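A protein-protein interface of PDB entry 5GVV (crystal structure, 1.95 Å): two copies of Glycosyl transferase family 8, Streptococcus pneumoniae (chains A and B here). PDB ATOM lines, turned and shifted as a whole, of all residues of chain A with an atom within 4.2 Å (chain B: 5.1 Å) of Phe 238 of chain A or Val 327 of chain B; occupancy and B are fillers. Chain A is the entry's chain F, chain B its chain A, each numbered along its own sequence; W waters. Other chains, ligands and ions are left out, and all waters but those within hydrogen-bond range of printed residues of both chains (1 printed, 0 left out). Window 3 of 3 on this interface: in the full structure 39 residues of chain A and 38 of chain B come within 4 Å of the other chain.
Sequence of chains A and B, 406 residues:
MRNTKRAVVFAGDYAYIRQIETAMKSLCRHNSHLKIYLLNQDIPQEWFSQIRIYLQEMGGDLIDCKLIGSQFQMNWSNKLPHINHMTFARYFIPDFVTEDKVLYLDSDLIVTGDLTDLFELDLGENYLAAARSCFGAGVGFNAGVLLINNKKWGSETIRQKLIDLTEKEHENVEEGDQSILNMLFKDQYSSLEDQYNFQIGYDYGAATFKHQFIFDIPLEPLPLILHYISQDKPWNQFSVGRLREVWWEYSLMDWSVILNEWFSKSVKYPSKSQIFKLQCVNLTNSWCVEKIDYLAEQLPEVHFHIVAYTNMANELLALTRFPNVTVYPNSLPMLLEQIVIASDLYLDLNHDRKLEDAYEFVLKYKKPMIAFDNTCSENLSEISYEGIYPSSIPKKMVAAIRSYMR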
ATOM      1  N   ASN A 236      21.505  -6.097 -22.861  1.00  0.00           N
ATOM      2  CA  ASN A 236      22.799  -6.324 -23.502  1.00  0.00           C
ATOM      3  C   ASN A 236      23.754  -5.186 -23.165  1.00  0.00           C
ATOM      4  O   ASN A 236      23.312  -4.112 -22.744  1.00  0.00           O
ATOM      5  CB  ASN A 236      22.646  -6.429 -25.019  1.00  0.00           C
ATOM      6  CG  ASN A 236      21.878  -7.660 -25.451  1.00  0.00           C
ATOM      7  OD1 ASN A 236      21.935  -8.706 -24.802  1.00  0.00           O
ATOM      8  ND2 ASN A 236      21.177  -7.551 -26.577  1.00  0.00           N
ATOM      9  N   GLN A 237      25.056  -5.413 -23.349  1.00  0.00           N
ATOM     10  CA  GLN A 237      26.049  -4.366 -23.111  1.00  0.00           C
ATOM     11  C   GLN A 237      25.704  -3.129 -23.939  1.00  0.00           C
ATOM     12  O   GLN A 237      25.704  -2.004 -23.429  1.00  0.00           O
ATOM     13  CB  GLN A 237      27.465  -4.852 -23.439  1.00  0.00           C
ATOM     14  CG  GLN A 237      28.537  -3.759 -23.248  1.00  0.00           C
ATOM     15  CD  GLN A 237      29.956  -4.261 -23.404  1.00  0.00           C
ATOM     16  OE1 GLN A 237      30.230  -5.169 -24.190  1.00  0.00           O
ATOM     17  NE2 GLN A 237      30.871  -3.676 -22.641  1.00  0.00           N
ATOM     18  N   PHE A 238      25.380  -3.347 -25.210  1.00  0.00           N
ATOM     19  CA  PHE A 238      24.930  -2.261 -26.064  1.00  0.00           C
ATOM     20  C   PHE A 238      23.552  -2.569 -26.633  1.00  0.00           C
ATOM     21  O   PHE A 238      23.202  -3.735 -26.843  1.00  0.00           O
ATOM     22  CB  PHE A 238      25.916  -2.042 -27.210  1.00  0.00           C
ATOM     23  CG  PHE A 238      27.352  -1.939 -26.767  1.00  0.00           C
ATOM     24  CD1 PHE A 238      27.825  -0.786 -26.153  1.00  0.00           C
ATOM     25  CD2 PHE A 238      28.234  -2.987 -26.992  1.00  0.00           C
ATOM     26  CE1 PHE A 238      29.157  -0.685 -25.754  1.00  0.00           C
ATOM     27  CE2 PHE A 238      29.561  -2.898 -26.600  1.00  0.00           C
ATOM     28  CZ  PHE A 238      30.025  -1.745 -25.982  1.00  0.00           C
ATOM     29  N   SER A 239      22.771  -1.519 -26.866  1.00  0.00           N
ATOM     30  CA  SER A 239      21.507  -1.634 -27.585  1.00  0.00           C
ATOM     31  C   SER A 239      21.212  -0.267 -28.196  1.00  0.00           C
ATOM     32  O   SER A 239      21.904   0.710 -27.892  1.00  0.00           O
ATOM     33  CB  SER A 239      20.371  -2.102 -26.662  1.00  0.00           C
ATOM     34  OG  SER A 239      20.085  -1.154 -25.643  1.00  0.00           O
ATOM     35  N   ARG A 244      15.610   1.811 -22.648  1.00  0.00           N
ATOM     36  CA  ARG A 244      16.558   0.863 -22.075  1.00  0.00           C
ATOM     37  C   ARG A 244      16.611   1.010 -20.556  1.00  0.00           C
ATOM     38  O   ARG A 244      16.682   0.013 -19.826  1.00  0.00           O
ATOM     39  CB  ARG A 244      17.945   1.078 -22.678  1.00  0.00           C
ATOM     40  CG  ARG A 244      19.043   0.258 -22.015  1.00  0.00           C
ATOM     41  CD  ARG A 244      20.408   0.635 -22.554  1.00  0.00           C
ATOM     42  NE  ARG A 244      21.490   0.024 -21.781  1.00  0.00           N
ATOM     43  CZ  ARG A 244      22.132  -1.087 -22.131  1.00  0.00           C
ATOM     44  NH1 ARG A 244      21.803  -1.733 -23.244  1.00  0.00           N
ATOM     45  NH2 ARG A 244      23.106  -1.558 -21.360  1.00  0.00           N
ATOM     46  N   ILE B 306      27.535   8.883 -27.863  1.00  0.00           N
ATOM     47  CA  ILE B 306      28.312   8.729 -29.090  1.00  0.00           C
ATOM     48  C   ILE B 306      27.654   7.673 -29.965  1.00  0.00           C
ATOM     49  O   ILE B 306      27.574   6.501 -29.583  1.00  0.00           O
ATOM     50  CB  ILE B 306      29.776   8.341 -28.802  1.00  0.00           C
ATOM     51  CG1 ILE B 306      30.388   9.289 -27.768  1.00  0.00           C
ATOM     52  CG2 ILE B 306      30.594   8.366 -30.091  1.00  0.00           C
ATOM     53  CD1 ILE B 306      30.308  10.762 -28.166  1.00  0.00           C
ATOM     54  N   MET B 312      31.935  -0.392 -33.998  1.00  0.00           N
ATOM     55  CA  MET B 312      32.846   0.603 -33.440  1.00  0.00           C
ATOM     56  C   MET B 312      34.187  -0.012 -33.061  1.00  0.00           C
ATOM     57  O   MET B 312      34.266  -1.183 -32.686  1.00  0.00           O
ATOM     58  CB  MET B 312      32.228   1.286 -32.217  1.00  0.00           C
ATOM     59  CG  MET B 312      31.129   2.304 -32.521  1.00  0.00           C
ATOM     60  SD  MET B 312      30.438   2.942 -30.820  1.00  0.00           S
ATOM     61  CE  MET B 312      29.339   4.436 -31.417  1.00  0.00           C
ATOM     62  N   LEU B 316      36.491   3.350 -28.972  1.00  0.00           N
ATOM     63  CA  LEU B 316      35.173   3.863 -28.616  1.00  0.00           C
ATOM     64  C   LEU B 316      34.439   2.915 -27.666  1.00  0.00           C
ATOM     65  O   LEU B 316      33.741   3.363 -26.756  1.00  0.00           O
ATOM     66  CB  LEU B 316      34.328   4.115 -29.873  1.00  0.00           C
ATOM     67  CG  LEU B 316      34.814   5.213 -30.821  1.00  0.00           C
ATOM     68  CD1 LEU B 316      33.829   5.419 -31.952  1.00  0.00           C
ATOM     69  CD2 LEU B 316      35.026   6.515 -30.078  1.00  0.00           C
ATOM     70  N   LEU B 317      34.592   1.609 -27.873  1.00  0.00           N
ATOM     71  CA  LEU B 317      33.931   0.637 -27.005  1.00  0.00           C
ATOM     72  C   LEU B 317      34.488   0.727 -25.592  1.00  0.00           C
ATOM     73  O   LEU B 317      33.756   0.553 -24.621  1.00  0.00           O
ATOM     74  CB  LEU B 317      34.071  -0.785 -27.554  1.00  0.00           C
ATOM     75  CG  LEU B 317      33.386  -1.063 -28.893  1.00  0.00           C
ATOM     76  CD1 LEU B 317      33.573  -2.519 -29.310  1.00  0.00           C
ATOM     77  CD2 LEU B 317      31.914  -0.721 -28.828  1.00  0.00           C
ATOM     78  N   LEU B 319      35.137   3.213 -24.015  1.00  0.00           N
ATOM     79  CA  LEU B 319      34.533   4.352 -23.326  1.00  0.00           C
ATOM     80  C   LEU B 319      33.483   3.915 -22.298  1.00  0.00           C
ATOM     81  O   LEU B 319      33.032   4.728 -21.491  1.00  0.00           O
ATOM     82  CB  LEU B 319      33.922   5.335 -24.330  1.00  0.00           C
ATOM     83  CG  LEU B 319      34.867   6.038 -25.307  1.00  0.00           C
ATOM     84  CD1 LEU B 319      34.095   6.895 -26.303  1.00  0.00           C
ATOM     85  CD2 LEU B 319      35.894   6.883 -24.554  1.00  0.00           C
ATOM     86  N   THR B 320      33.095   2.639 -22.331  1.00  0.00           N
ATOM     87  CA  THR B 320      32.168   2.078 -21.343  1.00  0.00           C
ATOM     88  C   THR B 320      32.725   2.067 -19.915  1.00  0.00           C
ATOM     89  O   THR B 320      31.983   1.837 -18.957  1.00  0.00           O
ATOM     90  CB  THR B 320      31.748   0.640 -21.709  1.00  0.00           C
ATOM     91  OG1 THR B 320      32.910  -0.189 -21.862  1.00  0.00           O
ATOM     92  CG2 THR B 320      30.946   0.625 -22.995  1.00  0.00           C
ATOM     93  N   VAL B 325      29.406   8.056 -20.319  1.00  0.00           N
ATOM     94  CA  VAL B 325      29.418   7.953 -21.777  1.00  0.00           C
ATOM     95  C   VAL B 325      28.541   6.796 -22.215  1.00  0.00           C
ATOM     96  O   VAL B 325      28.717   5.660 -21.753  1.00  0.00           O
ATOM     97  CB  VAL B 325      30.837   7.725 -22.335  1.00  0.00           C
ATOM     98  CG1 VAL B 325      30.798   7.662 -23.859  1.00  0.00           C
ATOM     99  CG2 VAL B 325      31.784   8.828 -21.875  1.00  0.00           C
ATOM    100  N   THR B 326      27.585   7.079 -23.091  1.00  0.00           N
ATOM    101  CA  THR B 326      26.826   6.006 -23.723  1.00  0.00           C
ATOM    102  C   THR B 326      27.204   5.918 -25.193  1.00  0.00           C
ATOM    103  O   THR B 326      27.251   6.925 -25.906  1.00  0.00           O
ATOM    104  CB  THR B 326      25.314   6.157 -23.523  1.00  0.00           C
ATOM    105  OG1 THR B 326      25.030   6.137 -22.117  1.00  0.00           O
ATOM    106  CG2 THR B 326      24.563   5.002 -24.182  1.00  0.00           C
ATOM    107  N   VAL B 327      27.494   4.694 -25.615  1.00  0.00           N
ATOM    108  CA  VAL B 327      28.047   4.382 -26.920  1.00  0.00           C
ATOM    109  C   VAL B 327      27.031   3.510 -27.679  1.00  0.00           C
ATOM    110  O   VAL B 327      26.544   2.513 -27.137  1.00  0.00           O
ATOM    111  CB  VAL B 327      29.394   3.666 -26.694  1.00  0.00           C
ATOM    112  CG1 VAL B 327      29.570   2.466 -27.593  1.00  0.00           C
ATOM    113  CG2 VAL B 327      30.560   4.654 -26.815  1.00  0.00           C
ATOM    114  N   TYR B 328      26.678   3.898 -28.907  1.00  0.00           N
ATOM    115  CA  TYR B 328      25.619   3.205 -29.642  1.00  0.00           C
ATOM    116  C   TYR B 328      26.095   2.669 -30.988  1.00  0.00           C
ATOM    117  O   TYR B 328      25.767   3.244 -32.031  1.00  0.00           O
ATOM    118  CB  TYR B 328      24.445   4.145 -29.925  1.00  0.00           C
ATOM    119  CG  TYR B 328      23.839   4.860 -28.739  1.00  0.00           C
ATOM    120  CD1 TYR B 328      24.401   6.037 -28.252  1.00  0.00           C
ATOM    121  CD2 TYR B 328      22.675   4.393 -28.142  1.00  0.00           C
ATOM    122  CE1 TYR B 328      23.836   6.711 -27.189  1.00  0.00           C
ATOM    123  CE2 TYR B 328      22.106   5.056 -27.070  1.00  0.00           C
ATOM    124  CZ  TYR B 328      22.687   6.219 -26.606  1.00  0.00           C
ATOM    125  OH  TYR B 328      22.132   6.900 -25.541  1.00  0.00           O
ATOM    126  N   PRO B 329      26.847   1.560 -30.985  1.00  0.00           N
ATOM    127  CA  PRO B 329      27.273   1.037 -32.285  1.00  0.00           C
ATOM    128  C   PRO B 329      26.076   0.504 -33.070  1.00  0.00           C
ATOM    129  O   PRO B 329      25.063   0.142 -32.461  1.00  0.00           O
ATOM    130  CB  PRO B 329      28.214  -0.111 -31.909  1.00  0.00           C
ATOM    131  CG  PRO B 329      27.735  -0.569 -30.546  1.00  0.00           C
ATOM    132  CD  PRO B 329      27.252   0.689 -29.862  1.00  0.00           C
HETATM  133  O   HOH W   1      24.136   1.200 -26.343  1.00  0.00           O
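No position is printed for both chains.
Of the 4 pairs that touch across the chains among the printed residues, none has its exchanged pair printed and touching as well.
Water W1 lies within hydrogen-bond range of the backbone carbonyl oxygen (O) of Ser 239 of chain A (2.8 Å) and the backbone carbonyl oxygen (O) of Val 327 of chain B (2.9 Å).
Of the 5 printed residues of chain A, 2 touch a printed residue of chain B.
Hydrophobic or aromatic side chains of chain A that line the printed part of chain B: Phe 238.
Printed residues of chain B that touch a printed residue of chain A: Leu 317, Thr 320, Val 327 and Tyr 328.
Hydrophobic or aromatic side chains of chain B that line the printed part of chain A: Leu 317, Val 327 and Tyr 328.
Among the printed residues, no Asp or Glu carboxylate lies within 4 Å of a Lys or Arg side-chain nitrogen of the other chain.
Asn 236 of chain A touches none of the printed residues of chain B.
Phe 238 of chain A touches just these residues of chain B: Leu 317, Thr 320 and Val 327.
Of the printed residues of chain A, Leu 317 of chain B touches Phe 238.
Of the printed residues of chain A, Thr 320 of chain B touches Phe 238 (3.5 Å).
Val 327 of chain B touches one residue of chain A.
Of the printed residues of chain A, Tyr 328 of chain B touches Ser 239.
The nearest residue of chain B that does not touch Phe 238 of chain A is Pro 329 of chain B (4.03 Å).
The nearest printed residue of chain A that does not touch Val 327 of chain B is Ser 239 of chain A (5.0 Å).
The nearest printed residue of chain B that does not touch Ser 239 of chain A is Val 327 of chain B (5.0 Å).
Among the printed residues, merely in contact across the chains: Phe 238 of chain A with Thr 320 of chain B, Phe 238 of chain A with Leu 317 of chain B, Phe 238 of chain A with Val 327 of chain B and Ser 239 of chain A with Tyr 328 of chain B.
The backbone carbonyl oxygen (O) of Ile 306 of chain B is in hydrogen-bond range of the backbone NH (N) of Tyr 328 of chain B (2.8 Å).
O of Leu 317 of chain B lies within hydrogen-bond range of OG1 of Thr 320 of chain B, at 3.0 Å.
OG of Ser 239 of chain A sits at hydrogen-bond distance from NH1 of Arg 244 of chain A (3.0 Å).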
